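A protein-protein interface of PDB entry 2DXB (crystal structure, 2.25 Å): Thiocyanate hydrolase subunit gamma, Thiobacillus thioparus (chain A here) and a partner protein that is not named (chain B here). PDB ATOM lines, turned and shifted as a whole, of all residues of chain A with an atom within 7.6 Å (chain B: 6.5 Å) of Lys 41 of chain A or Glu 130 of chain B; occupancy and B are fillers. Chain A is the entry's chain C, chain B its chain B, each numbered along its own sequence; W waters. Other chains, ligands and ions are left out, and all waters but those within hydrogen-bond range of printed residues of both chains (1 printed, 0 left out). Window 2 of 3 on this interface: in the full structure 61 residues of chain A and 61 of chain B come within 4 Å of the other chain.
NZ of Lys 134 of chain B lies within salt-bridge range of OE2 of Glu 40 of chain A (2.7 Å). The side-chain amino group (NZ) of Lys 134 of chain B is in salt-bridge range of the side-chain carboxylate (OE1) of Glu 36 of chain A (3.0 Å). NZ of Lys 41 of chain A lies within salt-bridge range of OE2 of Glu 130 of chain B.
O of Ala 38 of chain A lies within hydrogen-bond range of N of Leu 43 of chain A, 2.9 Å away. The side-chain carboxylate (OE1) of Glu 130 of chain B sits at hydrogen-bond distance from the backbone NH (N) of Thr 127 of chain B (2.9 Å).
Ala 33 of chain A touches Lys 134 of chain B. Ala 33 of chain A touches Ile 135 of chain B. Leu 37 of chain A touches Leu 131 of chain B. Leu 37 of chain A touches Lys 134 of chain B (CD2 to CE, 3.8 Å). Lys 41 of chain A touches Phe 125 of chain B. CG1 of Val 126 of chain B touches CG of Lys 41 of chain A, at 3.7 Å. Leu 43 of chain A touches Phe 125 of chain B.
Printed residues of chain B within 4 Å of Glu 36 of chain A: Lys 134. Of the printed residues of chain B, Leu 37 of chain A touches Leu 131 (3.8 Å) and Lys 134 (3.8 Å). Of the printed residues of chain B, Glu 40 of chain A touches Lys 134. Printed residues of chain B within 4 Å of Leu 43 of chain A: Phe 125. Of the printed residues of chain A, Val 126 of chain B touches Lys 41. Glu 130 of chain B touches just one residue of chain A: Lys 41 (2.8 Å). The nearest residue of chain A that does not touch Glu 130 of chain B is Leu 37 of chain A (4.2 Å).
Hydrophobic or aromatic side chains of chain A that line the printed part of chain B: Ala 33, Leu 37 and Leu 43. Along chain A the printed residues that touch a printed residue of chain B span positions 33 to 43. Printed residues of chain B that touch a printed residue of chain A: Phe 125, Val 126, Glu 130, Leu 131, Lys 134 and Ile 135. Hydrophobic or aromatic side chains of chain B within 4 Å of the printed part of chain A: Phe 125, Val 126, Leu 131 and Ile 135. Among the printed residues, 10 pairs touch across the chains.
Water W1 bridges the side-chain carboxylate of Glu 130 of chain B and the side-chain amino group of Lys 41 of chain A.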
ATOM      1  N   ALA A  33       9.865  31.540  14.333  1.00  0.00           N
ATOM      2  CA  ALA A  33      10.020  30.091  14.295  1.00  0.00           C
ATOM      3  C   ALA A  33       9.967  29.544  12.871  1.00  0.00           C
ATOM      4  O   ALA A  33      10.837  28.774  12.460  1.00  0.00           O
ATOM      5  CB  ALA A  33       8.943  29.430  15.151  1.00  0.00           C
ATOM      6  N   ARG A  35      10.309  31.187   9.902  1.00  0.00           N
ATOM      7  CA  ARG A  35      11.384  31.721   9.071  1.00  0.00           C
ATOM      8  C   ARG A  35      12.722  31.050   9.367  1.00  0.00           C
ATOM      9  O   ARG A  35      13.438  30.650   8.448  1.00  0.00           O
ATOM     10  CB  ARG A  35      11.493  33.241   9.260  1.00  0.00           C
ATOM     11  CG  ARG A  35      12.678  33.882   8.550  1.00  0.00           C
ATOM     12  CD  ARG A  35      12.359  35.303   8.085  1.00  0.00           C
ATOM     13  NE  ARG A  35      11.797  36.138   9.143  1.00  0.00           N
ATOM     14  CZ  ARG A  35      12.486  36.631  10.167  1.00  0.00           C
ATOM     15  NH1 ARG A  35      13.784  36.381  10.282  1.00  0.00           N
ATOM     16  NH2 ARG A  35      11.875  37.372  11.081  1.00  0.00           N
ATOM     17  N   GLU A  36      13.059  30.928  10.645  1.00  0.00           N
ATOM     18  CA  GLU A  36      14.313  30.286  11.018  1.00  0.00           C
ATOM     19  C   GLU A  36      14.329  28.825  10.586  1.00  0.00           C
ATOM     20  O   GLU A  36      15.340  28.332  10.088  1.00  0.00           O
ATOM     21  CB  GLU A  36      14.549  30.393  12.526  1.00  0.00           C
ATOM     22  CG  GLU A  36      15.372  31.615  12.907  1.00  0.00           C
ATOM     23  CD  GLU A  36      15.651  31.706  14.394  1.00  0.00           C
ATOM     24  OE1 GLU A  36      15.856  30.651  15.033  1.00  0.00           O
ATOM     25  OE2 GLU A  36      15.683  32.841  14.916  1.00  0.00           O
ATOM     26  N   LEU A  37      13.208  28.134  10.764  1.00  0.00           N
ATOM     27  CA  LEU A  37      13.142  26.735  10.368  1.00  0.00           C
ATOM     28  C   LEU A  37      13.279  26.585   8.855  1.00  0.00           C
ATOM     29  O   LEU A  37      14.028  25.733   8.379  1.00  0.00           O
ATOM     30  CB  LEU A  37      11.834  26.094  10.848  1.00  0.00           C
ATOM     31  CG  LEU A  37      11.778  25.691  12.327  1.00  0.00           C
ATOM     32  CD1 LEU A  37      10.388  25.177  12.673  1.00  0.00           C
ATOM     33  CD2 LEU A  37      12.816  24.615  12.605  1.00  0.00           C
ATOM     34  N   ALA A  38      12.567  27.418   8.100  1.00  0.00           N
ATOM     35  CA  ALA A  38      12.626  27.351   6.641  1.00  0.00           C
ATOM     36  C   ALA A  38      14.053  27.573   6.128  1.00  0.00           C
ATOM     37  O   ALA A  38      14.518  26.871   5.225  1.00  0.00           O
ATOM     38  CB  ALA A  38      11.684  28.388   6.031  1.00  0.00           C
ATOM     39  N   ILE A  39      14.746  28.546   6.712  1.00  0.00           N
ATOM     40  CA  ILE A  39      16.111  28.857   6.308  1.00  0.00           C
ATOM     41  C   ILE A  39      17.058  27.733   6.699  1.00  0.00           C
ATOM     42  O   ILE A  39      17.894  27.315   5.897  1.00  0.00           O
ATOM     43  CB  ILE A  39      16.583  30.182   6.936  1.00  0.00           C
ATOM     44  CG1 ILE A  39      15.737  31.334   6.384  1.00  0.00           C
ATOM     45  CG2 ILE A  39      18.058  30.419   6.623  1.00  0.00           C
ATOM     46  CD1 ILE A  39      16.043  32.694   6.997  1.00  0.00           C
ATOM     47  N   GLU A  40      16.919  27.238   7.927  1.00  0.00           N
ATOM     48  CA  GLU A  40      17.748  26.139   8.421  1.00  0.00           C
ATOM     49  C   GLU A  40      17.652  24.918   7.521  1.00  0.00           C
ATOM     50  O   GLU A  40      18.651  24.257   7.250  1.00  0.00           O
ATOM     51  CB  GLU A  40      17.317  25.731   9.828  1.00  0.00           C
ATOM     52  CG  GLU A  40      17.860  26.603  10.937  1.00  0.00           C
ATOM     53  CD  GLU A  40      17.140  26.365  12.252  1.00  0.00           C
ATOM     54  OE1 GLU A  40      16.914  25.184  12.607  1.00  0.00           O
ATOM     55  OE2 GLU A  40      16.807  27.360  12.933  1.00  0.00           O
ATOM     56  N   LYS A  41      16.441  24.616   7.068  1.00  0.00           N
ATOM     57  CA  LYS A  41      16.210  23.458   6.213  1.00  0.00           C
ATOM     58  C   LYS A  41      16.539  23.731   4.749  1.00  0.00           C
ATOM     59  O   LYS A  41      16.373  22.865   3.897  1.00  0.00           O
ATOM     60  CB  LYS A  41      14.755  22.999   6.342  1.00  0.00           C
ATOM     61  CG  LYS A  41      14.363  22.584   7.757  1.00  0.00           C
ATOM     62  CD  LYS A  41      15.188  21.396   8.249  1.00  0.00           C
ATOM     63  CE  LYS A  41      14.759  20.960   9.644  1.00  0.00           C
ATOM     64  NZ  LYS A  41      15.497  19.750  10.124  1.00  0.00           N
ATOM     65  N   GLY A  42      17.000  24.943   4.462  1.00  0.00           N
ATOM     66  CA  GLY A  42      17.354  25.297   3.098  1.00  0.00           C
ATOM     67  C   GLY A  42      16.186  25.428   2.135  1.00  0.00           C
ATOM     68  O   GLY A  42      16.351  25.213   0.936  1.00  0.00           O
ATOM     69  N   LEU A  43      15.006  25.778   2.638  1.00  0.00           N
ATOM     70  CA  LEU A  43      13.851  25.929   1.762  1.00  0.00           C
ATOM     71  C   LEU A  43      14.013  27.212   0.951  1.00  0.00           C
ATOM     72  O   LEU A  43      13.685  27.254  -0.232  1.00  0.00           O
ATOM     73  CB  LEU A  43      12.560  25.928   2.583  1.00  0.00           C
ATOM     74  CG  LEU A  43      12.366  24.617   3.357  1.00  0.00           C
ATOM     75  CD1 LEU A  43      11.023  24.633   4.052  1.00  0.00           C
ATOM     76  CD2 LEU A  43      12.450  23.423   2.411  1.00  0.00           C
ATOM     77  N   PHE A  44      14.507  28.259   1.604  1.00  0.00           N
ATOM     78  CA  PHE A  44      14.815  29.526   0.946  1.00  0.00           C
ATOM     79  C   PHE A  44      15.886  30.176   1.817  1.00  0.00           C
ATOM     80  O   PHE A  44      16.059  29.790   2.968  1.00  0.00           O
ATOM     81  CB  PHE A  44      13.570  30.429   0.759  1.00  0.00           C
ATOM     82  CG  PHE A  44      12.938  30.919   2.038  1.00  0.00           C
ATOM     83  CD1 PHE A  44      13.566  31.879   2.827  1.00  0.00           C
ATOM     84  CD2 PHE A  44      11.685  30.454   2.423  1.00  0.00           C
ATOM     85  CE1 PHE A  44      12.955  32.376   3.985  1.00  0.00           C
ATOM     86  CE2 PHE A  44      11.059  30.938   3.577  1.00  0.00           C
ATOM     87  CZ  PHE A  44      11.696  31.904   4.360  1.00  0.00           C
ATOM     88  N   PHE B 125       9.162  18.771   5.873  1.00  0.00           N
ATOM     89  CA  PHE B 125      10.446  19.465   5.768  1.00  0.00           C
ATOM     90  C   PHE B 125      10.959  19.700   7.186  1.00  0.00           C
ATOM     91  O   PHE B 125      12.146  19.935   7.406  1.00  0.00           O
ATOM     92  CB  PHE B 125      10.297  20.791   5.017  1.00  0.00           C
ATOM     93  CG  PHE B 125      10.111  20.620   3.544  1.00  0.00           C
ATOM     94  CD1 PHE B 125      11.084  19.978   2.781  1.00  0.00           C
ATOM     95  CD2 PHE B 125       8.952  21.064   2.917  1.00  0.00           C
ATOM     96  CE1 PHE B 125      10.902  19.777   1.411  1.00  0.00           C
ATOM     97  CE2 PHE B 125       8.761  20.869   1.548  1.00  0.00           C
ATOM     98  CZ  PHE B 125       9.739  20.222   0.796  1.00  0.00           C
ATOM     99  N   VAL B 126      10.031  19.644   8.135  1.00  0.00           N
ATOM    100  CA  VAL B 126      10.331  19.770   9.555  1.00  0.00           C
ATOM    101  C   VAL B 126       9.308  18.876  10.246  1.00  0.00           C
ATOM    102  O   VAL B 126       8.197  18.699   9.743  1.00  0.00           O
ATOM    103  CB  VAL B 126      10.151  21.217  10.093  1.00  0.00           C
ATOM    104  CG1 VAL B 126      11.047  22.181   9.335  1.00  0.00           C
ATOM    105  CG2 VAL B 126       8.692  21.641   9.987  1.00  0.00           C
ATOM    106  N   THR B 127       9.680  18.285  11.373  1.00  0.00           N
ATOM    107  CA  THR B 127       8.736  17.450  12.101  1.00  0.00           C
ATOM    108  C   THR B 127       7.930  18.397  12.986  1.00  0.00           C
ATOM    109  O   THR B 127       8.373  19.513  13.265  1.00  0.00           O
ATOM    110  CB  THR B 127       9.451  16.435  13.006  1.00  0.00           C
ATOM    111  OG1 THR B 127      10.268  17.138  13.950  1.00  0.00           O
ATOM    112  CG2 THR B 127      10.315  15.495  12.178  1.00  0.00           C
ATOM    113  N   LEU B 128       6.752  17.970  13.421  1.00  0.00           N
ATOM    114  CA  LEU B 128       5.954  18.828  14.287  1.00  0.00           C
ATOM    115  C   LEU B 128       6.781  19.063  15.547  1.00  0.00           C
ATOM    116  O   LEU B 128       6.708  20.129  16.172  1.00  0.00           O
ATOM    117  CB  LEU B 128       4.620  18.156  14.639  1.00  0.00           C
ATOM    118  CG  LEU B 128       3.672  18.973  15.529  1.00  0.00           C
ATOM    119  CD1 LEU B 128       3.394  20.322  14.879  1.00  0.00           C
ATOM    120  CD2 LEU B 128       2.374  18.207  15.746  1.00  0.00           C
ATOM    121  N   THR B 129       7.585  18.061  15.898  1.00  0.00           N
ATOM    122  CA  THR B 129       8.441  18.130  17.078  1.00  0.00           C
ATOM    123  C   THR B 129       9.425  19.293  16.963  1.00  0.00           C
ATOM    124  O   THR B 129       9.635  20.034  17.922  1.00  0.00           O
ATOM    125  CB  THR B 129       9.224  16.806  17.269  1.00  0.00           C
ATOM    126  OG1 THR B 129       8.298  15.722  17.402  1.00  0.00           O
ATOM    127  CG2 THR B 129      10.097  16.867  18.522  1.00  0.00           C
ATOM    128  N   GLU B 130      10.023  19.454  15.787  1.00  0.00           N
ATOM    129  CA  GLU B 130      10.976  20.540  15.570  1.00  0.00           C
ATOM    130  C   GLU B 130      10.271  21.887  15.654  1.00  0.00           C
ATOM    131  O   GLU B 130      10.823  22.849  16.189  1.00  0.00           O
ATOM    132  CB  GLU B 130      11.659  20.398  14.207  1.00  0.00           C
ATOM    133  CG  GLU B 130      12.577  19.196  14.103  1.00  0.00           C
ATOM    134  CD  GLU B 130      13.218  19.068  12.729  1.00  0.00           C
ATOM    135  OE1 GLU B 130      12.483  18.921  11.732  1.00  0.00           O
ATOM    136  OE2 GLU B 130      14.462  19.120  12.645  1.00  0.00           O
ATOM    137  N   LEU B 131       9.049  21.958  15.132  1.00  0.00           N
ATOM    138  CA  LEU B 131       8.295  23.209  15.180  1.00  0.00           C
ATOM    139  C   LEU B 131       7.934  23.564  16.621  1.00  0.00           C
ATOM    140  O   LEU B 131       8.076  24.713  17.040  1.00  0.00           O
ATOM    141  CB  LEU B 131       7.020  23.106  14.339  1.00  0.00           C
ATOM    142  CG  LEU B 131       6.074  24.313  14.409  1.00  0.00           C
ATOM    143  CD1 LEU B 131       6.817  25.592  14.050  1.00  0.00           C
ATOM    144  CD2 LEU B 131       4.896  24.096  13.462  1.00  0.00           C
ATOM    145  N   HIS B 132       7.462  22.580  17.379  1.00  0.00           N
ATOM    146  CA  HIS B 132       7.102  22.828  18.769  1.00  0.00           C
ATOM    147  C   HIS B 132       8.347  23.258  19.555  1.00  0.00           C
ATOM    148  O   HIS B 132       8.291  24.181  20.372  1.00  0.00           O
ATOM    149  CB  HIS B 132       6.484  21.570  19.393  1.00  0.00           C
ATOM    150  CG  HIS B 132       5.087  21.283  18.927  1.00  0.00           C
ATOM    151  ND1 HIS B 132       4.393  20.155  19.312  1.00  0.00           N
ATOM    152  CD2 HIS B 132       4.246  21.988  18.131  1.00  0.00           C
ATOM    153  CE1 HIS B 132       3.185  20.178  18.775  1.00  0.00           C
ATOM    154  NE2 HIS B 132       3.071  21.280  18.054  1.00  0.00           N
ATOM    155  N   ASN B 133       9.474  22.598  19.298  1.00  0.00           N
ATOM    156  CA  ASN B 133      10.713  22.941  19.985  1.00  0.00           C
ATOM    157  C   ASN B 133      11.213  24.318  19.566  1.00  0.00           C
ATOM    158  O   ASN B 133      11.793  25.048  20.374  1.00  0.00           O
ATOM    159  CB  ASN B 133      11.796  21.897  19.710  1.00  0.00           C
ATOM    160  CG  ASN B 133      11.470  20.546  20.317  1.00  0.00           C
ATOM    161  OD1 ASN B 133      10.665  20.449  21.243  1.00  0.00           O
ATOM    162  ND2 ASN B 133      12.105  19.498  19.807  1.00  0.00           N
ATOM    163  N   LYS B 134      10.997  24.677  18.306  1.00  0.00           N
ATOM    164  CA  LYS B 134      11.433  25.983  17.837  1.00  0.00           C
ATOM    165  C   LYS B 134      10.608  27.063  18.535  1.00  0.00           C
ATOM    166  O   LYS B 134      11.133  28.119  18.889  1.00  0.00           O
ATOM    167  CB  LYS B 134      11.284  26.090  16.315  1.00  0.00           C
ATOM    168  CG  LYS B 134      11.661  27.453  15.759  1.00  0.00           C
ATOM    169  CD  LYS B 134      13.114  27.823  16.041  1.00  0.00           C
ATOM    170  CE  LYS B 134      14.084  27.082  15.134  1.00  0.00           C
ATOM    171  NZ  LYS B 134      15.449  27.682  15.217  1.00  0.00           N
ATOM    172  N   ILE B 135       9.321  26.791  18.741  1.00  0.00           N
ATOM    173  CA  ILE B 135       8.448  27.745  19.420  1.00  0.00           C
ATOM    174  C   ILE B 135       8.972  27.969  20.836  1.00  0.00           C
ATOM    175  O   ILE B 135       9.053  29.107  21.307  1.00  0.00           O
ATOM    176  CB  ILE B 135       6.995  27.228  19.524  1.00  0.00           C
ATOM    177  CG1 ILE B 135       6.379  27.086  18.131  1.00  0.00           C
ATOM    178  CG2 ILE B 135       6.163  28.181  20.380  1.00  0.00           C
ATOM    179  CD1 ILE B 135       6.282  28.380  17.375  1.00  0.00           C
HETATM  180  O   HOH W   1      13.155  17.264   9.754  1.00  0.00           O
